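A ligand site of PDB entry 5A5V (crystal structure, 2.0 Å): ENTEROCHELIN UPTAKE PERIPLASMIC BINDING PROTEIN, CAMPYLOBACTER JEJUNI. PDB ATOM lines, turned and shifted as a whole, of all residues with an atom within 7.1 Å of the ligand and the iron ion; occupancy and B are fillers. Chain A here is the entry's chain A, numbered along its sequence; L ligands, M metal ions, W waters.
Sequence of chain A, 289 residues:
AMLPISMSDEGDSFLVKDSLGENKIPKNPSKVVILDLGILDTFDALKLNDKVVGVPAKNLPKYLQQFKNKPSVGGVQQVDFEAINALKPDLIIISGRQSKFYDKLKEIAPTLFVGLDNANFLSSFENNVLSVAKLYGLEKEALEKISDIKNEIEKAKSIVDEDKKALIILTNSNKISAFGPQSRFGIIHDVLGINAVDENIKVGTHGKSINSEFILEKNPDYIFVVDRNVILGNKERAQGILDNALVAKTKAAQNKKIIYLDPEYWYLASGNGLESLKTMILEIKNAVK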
ATOM      1  N   ASN A  59      -1.265 -27.794 -34.207  1.00  0.00           N
ATOM      2  CA  ASN A  59      -0.366 -26.683 -33.791  1.00  0.00           C
ATOM      3  C   ASN A  59       1.108 -26.826 -34.261  1.00  0.00           C
ATOM      4  O   ASN A  59       2.019 -26.412 -33.559  1.00  0.00           O
ATOM      5  CB  ASN A  59      -0.371 -26.582 -32.301  1.00  0.00           C
ATOM      6  CG  ASN A  59      -1.761 -26.500 -31.730  1.00  0.00           C
ATOM      7  OD1 ASN A  59      -2.233 -27.400 -31.014  1.00  0.00           O
ATOM      8  ND2 ASN A  59      -2.415 -25.426 -32.014  1.00  0.00           N
ATOM      9  N   GLY A  75      -3.920 -31.590 -31.378  1.00  0.00           N
ATOM     10  CA  GLY A  75      -3.342 -30.334 -30.946  1.00  0.00           C
ATOM     11  C   GLY A  75      -2.790 -30.439 -29.543  1.00  0.00           C
ATOM     12  O   GLY A  75      -3.076 -31.403 -28.836  1.00  0.00           O
ATOM     13  N   VAL A  76      -2.014 -29.449 -29.133  1.00  0.00           N
ATOM     14  CA  VAL A  76      -1.365 -29.498 -27.832  1.00  0.00           C
ATOM     15  C   VAL A  76      -2.368 -29.358 -26.686  1.00  0.00           C
ATOM     16  O   VAL A  76      -2.122 -29.858 -25.583  1.00  0.00           O
ATOM     17  CB  VAL A  76      -0.214 -28.472 -27.709  1.00  0.00           C
ATOM     18  CG1 VAL A  76       0.865 -28.798 -28.736  1.00  0.00           C
ATOM     19  CG2 VAL A  76      -0.720 -27.011 -27.814  1.00  0.00           C
ATOM     20  N   GLN A  77      -3.474 -28.705 -26.970  1.00  0.00           N
ATOM     21  CA  GLN A  77      -4.636 -28.581 -26.060  1.00  0.00           C
ATOM     22  C   GLN A  77      -5.814 -29.471 -26.489  1.00  0.00           C
ATOM     23  O   GLN A  77      -6.920 -29.311 -26.009  1.00  0.00           O
ATOM     24  CB  GLN A  77      -5.106 -27.105 -26.048  1.00  0.00           C
ATOM     25  CG  GLN A  77      -6.307 -26.786 -25.172  1.00  0.00           C
ATOM     26  OE1 GLN A  77      -2.929 -25.828 -24.059  1.00  0.00           O
ATOM     27  NE2 GLN A  77      -3.979 -27.614 -23.206  1.00  0.00           N
ATOM     28  N   GLN A  78      -5.576 -30.425 -27.375  1.00  0.00           N
ATOM     29  CA  GLN A  78      -6.666 -31.198 -27.992  1.00  0.00           C
ATOM     30  C   GLN A  78      -6.035 -32.508 -28.460  1.00  0.00           C
ATOM     31  O   GLN A  78      -5.907 -32.786 -29.661  1.00  0.00           O
ATOM     32  CB  GLN A  78      -7.201 -30.416 -29.195  1.00  0.00           C
ATOM     33  CG  GLN A  78      -8.691 -30.281 -29.322  1.00  0.00           C
ATOM     34  CD  GLN A  78      -9.043 -29.352 -30.475  1.00  0.00           C
ATOM     35  OE1 GLN A  78      -9.043 -28.116 -30.319  1.00  0.00           O
ATOM     36  NE2 GLN A  78      -9.301 -29.918 -31.639  1.00  0.00           N
ATOM     37  N   SER A  95       4.594 -32.106 -21.836  1.00  0.00           N
ATOM     38  CA  SER A  95       4.889 -31.046 -20.903  1.00  0.00           C
ATOM     39  C   SER A  95       3.600 -30.540 -20.281  1.00  0.00           C
ATOM     40  O   SER A  95       2.603 -31.243 -20.243  1.00  0.00           O
ATOM     41  CB  SER A  95       5.639 -29.909 -21.609  1.00  0.00           C
ATOM     42  OG  SER A  95       5.075 -29.606 -22.863  1.00  0.00           O
ATOM     43  N   GLY A  96       3.640 -29.303 -19.784  1.00  0.00           N
ATOM     44  CA  GLY A  96       2.639 -28.761 -18.890  1.00  0.00           C
ATOM     45  C   GLY A  96       1.229 -28.804 -19.416  1.00  0.00           C
ATOM     46  O   GLY A  96       0.306 -28.922 -18.631  1.00  0.00           O
ATOM     47  N   ARG A  97       1.061 -28.673 -20.726  1.00  0.00           N
ATOM     48  CA  ARG A  97      -0.257 -28.621 -21.307  1.00  0.00           C
ATOM     49  C   ARG A  97      -0.968 -29.967 -21.230  1.00  0.00           C
ATOM     50  O   ARG A  97      -2.173 -29.990 -21.191  1.00  0.00           O
ATOM     51  CB  ARG A  97      -0.200 -28.162 -22.758  1.00  0.00           C
ATOM     52  CG  ARG A  97       0.283 -26.727 -22.922  1.00  0.00           C
ATOM     53  CD  ARG A  97       0.157 -26.367 -24.405  1.00  0.00           C
ATOM     54  NE  ARG A  97       0.288 -24.947 -24.699  1.00  0.00           N
ATOM     55  CZ  ARG A  97       1.414 -24.340 -25.047  1.00  0.00           C
ATOM     56  NH1 ARG A  97       2.549 -24.999 -25.136  1.00  0.00           N
ATOM     57  NH2 ARG A  97       1.375 -23.052 -25.326  1.00  0.00           N
ATOM     58  N   GLN A  98      -0.223 -31.067 -21.187  1.00  0.00           N
ATOM     59  CA  GLN A  98      -0.830 -32.384 -21.059  1.00  0.00           C
ATOM     60  C   GLN A  98      -0.764 -33.074 -19.668  1.00  0.00           C
ATOM     61  O   GLN A  98      -1.307 -34.181 -19.481  1.00  0.00           O
ATOM     62  CB  GLN A  98      -0.275 -33.295 -22.140  1.00  0.00           C
ATOM     63  CG  GLN A  98      -0.363 -32.717 -23.525  1.00  0.00           C
ATOM     64  CD  GLN A  98       0.839 -31.861 -23.944  1.00  0.00           C
ATOM     65  OE1 GLN A  98       1.964 -32.060 -23.498  1.00  0.00           O
ATOM     66  NE2 GLN A  98       0.588 -30.899 -24.847  1.00  0.00           N
ATOM     67  N   SER A  99      -0.195 -32.405 -18.665  1.00  0.00           N
ATOM     68  CA  SER A  99      -0.064 -33.003 -17.319  1.00  0.00           C
ATOM     69  C   SER A  99      -1.329 -33.581 -16.752  1.00  0.00           C
ATOM     70  O   SER A  99      -1.275 -34.592 -16.022  1.00  0.00           O
ATOM     71  CB  SER A  99       0.424 -32.010 -16.248  1.00  0.00           C
ATOM     72  OG  SER A  99       1.650 -31.563 -16.621  1.00  0.00           O
ATOM     73  N   LYS A 100      -2.460 -32.966 -17.066  1.00  0.00           N
ATOM     74  CA  LYS A 100      -3.699 -33.420 -16.476  1.00  0.00           C
ATOM     75  C   LYS A 100      -4.145 -34.751 -17.099  1.00  0.00           C
ATOM     76  O   LYS A 100      -4.963 -35.425 -16.507  1.00  0.00           O
ATOM     77  CB  LYS A 100      -4.810 -32.329 -16.558  1.00  0.00           C
ATOM     78  CG  LYS A 100      -5.328 -31.999 -17.953  1.00  0.00           C
ATOM     79  CD  LYS A 100      -6.267 -30.786 -17.899  1.00  0.00           C
ATOM     80  CE  LYS A 100      -5.898 -29.726 -18.939  1.00  0.00           C
ATOM     81  NZ  LYS A 100      -4.489 -29.241 -18.786  1.00  0.00           N
ATOM     82  N   ARG A 184       6.497 -17.706 -17.815  1.00  0.00           N
ATOM     83  CA  ARG A 184       6.786 -18.586 -18.917  1.00  0.00           C
ATOM     84  C   ARG A 184       7.647 -17.928 -19.982  1.00  0.00           C
ATOM     85  O   ARG A 184       8.165 -18.647 -20.808  1.00  0.00           O
ATOM     86  CB  ARG A 184       5.506 -19.075 -19.570  1.00  0.00           C
ATOM     87  CG  ARG A 184       4.764 -17.988 -20.369  1.00  0.00           C
ATOM     88  CD  ARG A 184       3.340 -18.427 -20.745  1.00  0.00           C
ATOM     89  NE  ARG A 184       3.353 -19.513 -21.699  1.00  0.00           N
ATOM     90  CZ  ARG A 184       2.297 -20.273 -22.007  1.00  0.00           C
ATOM     91  NH1 ARG A 184       1.106 -20.054 -21.460  1.00  0.00           N
ATOM     92  NH2 ARG A 184       2.431 -21.289 -22.861  1.00  0.00           N
ATOM     93  N   THR A 205      -0.285 -18.663 -15.791  1.00  0.00           N
ATOM     94  CA  THR A 205      -0.058 -19.357 -17.046  1.00  0.00           C
ATOM     95  C   THR A 205      -0.352 -18.515 -18.253  1.00  0.00           C
ATOM     96  O   THR A 205       0.474 -18.451 -19.154  1.00  0.00           O
ATOM     97  CB  THR A 205      -0.909 -20.598 -17.144  1.00  0.00           C
ATOM     98  OG1 THR A 205      -0.743 -21.355 -15.967  1.00  0.00           O
ATOM     99  CG2 THR A 205      -0.570 -21.443 -18.391  1.00  0.00           C
ATOM    100  N   HIS A 206      -1.503 -17.862 -18.295  1.00  0.00           N
ATOM    101  CA  HIS A 206      -1.809 -16.912 -19.405  1.00  0.00           C
ATOM    102  C   HIS A 206      -1.804 -15.433 -18.994  1.00  0.00           C
ATOM    103  O   HIS A 206      -2.374 -14.591 -19.679  1.00  0.00           O
ATOM    104  CB  HIS A 206      -3.133 -17.261 -20.105  1.00  0.00           C
ATOM    105  CG  HIS A 206      -3.163 -18.640 -20.668  1.00  0.00           C
ATOM    106  ND1 HIS A 206      -3.660 -19.708 -19.958  1.00  0.00           N
ATOM    107  CD2 HIS A 206      -2.764 -19.135 -21.860  1.00  0.00           C
ATOM    108  CE1 HIS A 206      -3.575 -20.807 -20.687  1.00  0.00           C
ATOM    109  NE2 HIS A 206      -3.035 -20.484 -21.852  1.00  0.00           N
ATOM    110  N   ARG A 228      -0.743 -14.262 -29.184  1.00  0.00           N
ATOM    111  CA  ARG A 228      -1.381 -15.535 -29.054  1.00  0.00           C
ATOM    112  C   ARG A 228      -2.452 -15.739 -30.145  1.00  0.00           C
ATOM    113  O   ARG A 228      -2.720 -16.852 -30.537  1.00  0.00           O
ATOM    114  CB  ARG A 228      -2.032 -15.630 -27.670  1.00  0.00           C
ATOM    115  CG  ARG A 228      -2.480 -17.017 -27.301  1.00  0.00           C
ATOM    116  CD  ARG A 228      -2.809 -17.083 -25.815  1.00  0.00           C
ATOM    117  NE  ARG A 228      -3.434 -18.367 -25.424  1.00  0.00           N
ATOM    118  CZ  ARG A 228      -4.732 -18.619 -25.392  1.00  0.00           C
ATOM    119  NH1 ARG A 228      -5.592 -17.665 -25.699  1.00  0.00           N
ATOM    120  NH2 ARG A 228      -5.161 -19.803 -25.027  1.00  0.00           N
ATOM    121  N   ILE A 231      -1.321 -18.116 -32.791  1.00  0.00           N
ATOM    122  CA  ILE A 231      -1.407 -19.488 -32.399  1.00  0.00           C
ATOM    123  C   ILE A 231      -2.840 -20.003 -32.466  1.00  0.00           C
ATOM    124  O   ILE A 231      -3.067 -21.159 -32.775  1.00  0.00           O
ATOM    125  CB  ILE A 231      -0.868 -19.635 -30.949  1.00  0.00           C
ATOM    126  CG1 ILE A 231       0.636 -19.280 -30.864  1.00  0.00           C
ATOM    127  CG2 ILE A 231      -1.136 -21.009 -30.399  1.00  0.00           C
ATOM    128  CD1 ILE A 231       1.456 -19.590 -32.105  1.00  0.00           C
ATOM    129  N   LEU A 232      -3.827 -19.166 -32.138  1.00  0.00           N
ATOM    130  CA  LEU A 232      -5.180 -19.659 -32.048  1.00  0.00           C
ATOM    131  C   LEU A 232      -5.883 -19.633 -33.405  1.00  0.00           C
ATOM    132  O   LEU A 232      -6.972 -20.173 -33.523  1.00  0.00           O
ATOM    133  CB  LEU A 232      -6.001 -18.870 -31.012  1.00  0.00           C
ATOM    134  CG  LEU A 232      -5.995 -19.380 -29.566  1.00  0.00           C
ATOM    135  CD1 LEU A 232      -6.614 -20.775 -29.452  1.00  0.00           C
ATOM    136  CD2 LEU A 232      -4.593 -19.444 -29.033  1.00  0.00           C
ATOM    137  N   TYR A 267       5.486 -18.866 -27.325  1.00  0.00           N
ATOM    138  CA  TYR A 267       4.271 -19.363 -26.668  1.00  0.00           C
ATOM    139  C   TYR A 267       4.121 -20.892 -26.751  1.00  0.00           C
ATOM    140  O   TYR A 267       3.792 -21.577 -25.749  1.00  0.00           O
ATOM    141  CB  TYR A 267       3.035 -18.688 -27.278  1.00  0.00           C
ATOM    142  CG  TYR A 267       1.768 -19.071 -26.535  1.00  0.00           C
ATOM    143  CD1 TYR A 267       1.535 -18.632 -25.216  1.00  0.00           C
ATOM    144  CD2 TYR A 267       0.845 -19.934 -27.112  1.00  0.00           C
ATOM    145  CE1 TYR A 267       0.395 -19.037 -24.519  1.00  0.00           C
ATOM    146  CE2 TYR A 267      -0.299 -20.309 -26.434  1.00  0.00           C
ATOM    147  CZ  TYR A 267      -0.527 -19.867 -25.152  1.00  0.00           C
ATOM    148  OH  TYR A 267      -1.630 -20.318 -24.503  1.00  0.00           O
ATOM    149  N   LEU A 268       4.306 -21.420 -27.952  1.00  0.00           N
ATOM    150  CA  LEU A 268       4.116 -22.852 -28.236  1.00  0.00           C
ATOM    151  C   LEU A 268       5.316 -23.674 -27.779  1.00  0.00           C
ATOM    152  O   LEU A 268       5.177 -24.527 -26.886  1.00  0.00           O
ATOM    153  CB  LEU A 268       3.873 -23.082 -29.740  1.00  0.00           C
ATOM    154  CG  LEU A 268       2.433 -23.034 -30.197  1.00  0.00           C
ATOM    155  CD1 LEU A 268       2.414 -23.303 -31.695  1.00  0.00           C
ATOM    156  CD2 LEU A 268       1.575 -24.052 -29.456  1.00  0.00           C
ATOM    157  N   SER A 270       7.920 -22.553 -26.150  1.00  0.00           N
ATOM    158  CA  SER A 270       8.370 -22.072 -24.812  1.00  0.00           C
ATOM    159  C   SER A 270       9.875 -22.132 -24.573  1.00  0.00           C
ATOM    160  O   SER A 270      10.329 -22.171 -23.399  1.00  0.00           O
ATOM    161  CB  SER A 270       7.661 -22.839 -23.686  1.00  0.00           C
ATOM    162  OG  SER A 270       6.253 -22.729 -23.866  1.00  0.00           O
HETATM  163  C1  LIG L   1      -1.954 -23.640 -27.212  1.00  0.00           C
HETATM  164  C2  LIG L   1      -2.335 -23.127 -25.968  1.00  0.00           C
HETATM  165  C3  LIG L   1      -3.641 -22.863 -25.735  1.00  0.00           C
HETATM  166  C4  LIG L   1      -4.627 -23.109 -26.712  1.00  0.00           C
HETATM  167  C5  LIG L   1      -4.255 -23.661 -27.945  1.00  0.00           C
HETATM  168  C6  LIG L   1      -2.900 -23.914 -28.200  1.00  0.00           C
HETATM  169  C7  LIG L   1      -6.082 -22.906 -26.397  1.00  0.00           C
HETATM  170  O1  LIG L   1      -6.951 -23.067 -27.225  1.00  0.00           O
HETATM  171  N1  LIG L   1      -6.379 -22.653 -25.116  1.00  0.00           N
HETATM  172  C8  LIG L   1      -7.720 -22.359 -24.693  1.00  0.00           C
HETATM  173  C9  LIG L   1      -8.052 -22.632 -23.244  1.00  0.00           C
HETATM  174  C10 LIG L   1      -6.890 -23.139 -22.419  1.00  0.00           C
HETATM  175  C11 LIG L   1      -7.220 -24.256 -21.468  1.00  0.00           C
HETATM  176  C12 LIG L   1      -6.413 -25.479 -21.814  1.00  0.00           C
HETATM  177  C13 LIG L   1      -5.489 -25.902 -20.704  1.00  0.00           C
HETATM  178  N2  LIG L   1      -4.195 -25.296 -20.936  1.00  0.00           N
HETATM  179  C14 LIG L   1      -3.132 -25.571 -20.191  1.00  0.00           C
HETATM  180  O2  LIG L   1      -3.225 -26.360 -19.270  1.00  0.00           O
HETATM  181  C15 LIG L   1      -1.803 -24.872 -20.451  1.00  0.00           C
HETATM  182  C16 LIG L   1      -1.667 -23.842 -21.397  1.00  0.00           C
HETATM  183  C17 LIG L   1      -0.455 -23.210 -21.601  1.00  0.00           C
HETATM  184  C18 LIG L   1       0.653 -23.616 -20.861  1.00  0.00           C
HETATM  185  C19 LIG L   1       0.542 -24.651 -19.920  1.00  0.00           C
HETATM  186  C20 LIG L   1      -0.688 -25.276 -19.724  1.00  0.00           C
HETATM  187  O3  LIG L   1      -3.902 -22.332 -24.515  1.00  0.00           O
HETATM  188  O4  LIG L   1      -1.459 -22.866 -24.962  1.00  0.00           O
HETATM  189  O5  LIG L   1      -2.707 -23.375 -22.138  1.00  0.00           O
HETATM  190  O6  LIG L   1      -0.362 -22.184 -22.504  1.00  0.00           O
HETATM  191 FE    FE M   1      -2.116 -21.860 -23.445  1.00  0.00          FE
HETATM  192  O   HOH W   1      -8.987 -21.173 -27.317  1.00  0.00           O
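A nitrogen (N2) of the ligand sits close to the side-chain amide nitrogen of Gln 77. The guanidinium group (NH2) of Arg 228 sits close to an oxygen (O3) of the ligand (2.9 Å). An oxygen (O4) of the ligand sits close to the guanidinium group (NE) of Arg 97. The guanidinium group (NH1) of Arg 184 lies close to an oxygen (O6) of the ligand. The side-chain amino group of Lys 100 sits at hydrogen-bond distance from an oxygen (O2) of the ligand, at 3.2 Å.
O of Tyr 267 is in hydrogen-bond range of NH2 of Arg 184, 3.2 Å away. NE of Arg 228 lies close to OH of Tyr 267. The side-chain amide nitrogen (NE2) of Gln 98 lies within hydrogen-bond range of the backbone carbonyl oxygen (O) of Val 76. The side-chain amino group (NZ) of Lys 100 is in hydrogen-bond range of the backbone carbonyl oxygen (O) of Arg 97 (3.4 Å). OE1 of Gln 77 sits close to NE of Arg 97 (3.4 Å). O of Tyr 267 lies within hydrogen-bond range of OG of Ser 270, 3.3 Å away. O of Leu 268 sits at hydrogen-bond distance from NH1 of Arg 97 (3.2 Å). The backbone carbonyl oxygen (O) of Thr 205 lies within hydrogen-bond range of the guanidinium group (NH1) of Arg 184.
Merely in contact with the ligand: Val 76 (3.6 Å), Gly 96 (3.9 Å), Thr 205 (3.5 Å) and Leu 232 (3.2 Å). Hydrophobic or aromatic side chains within 4 Å of the ligand: Val 76, His 206, Leu 232 and Tyr 267. Within 4 Å of the ligand: Val 76, Gln 77, Gly 96, Arg 97, Lys 100, Arg 184, Thr 205, His 206, Arg 228, Leu 232 and Tyr 267. The nearest printed residue that does not touch the ligand is Ile 231 (4.05 Å).
Two residues have an atom within 4 Å of the iron ion: His 206 and Tyr 267. The nearest printed residue that does not touch the iron ion is Arg 228 (4.001 Å).
The iron ion is bound by OH of Tyr 267 (1.9 Å), O4 of the ligand (1.9 Å), O6 of the ligand (2.0 Å), O5 of the ligand (2.1 Å), O3 of the ligand (2.1 Å) and NE2 of His 206 (2.3 Å).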
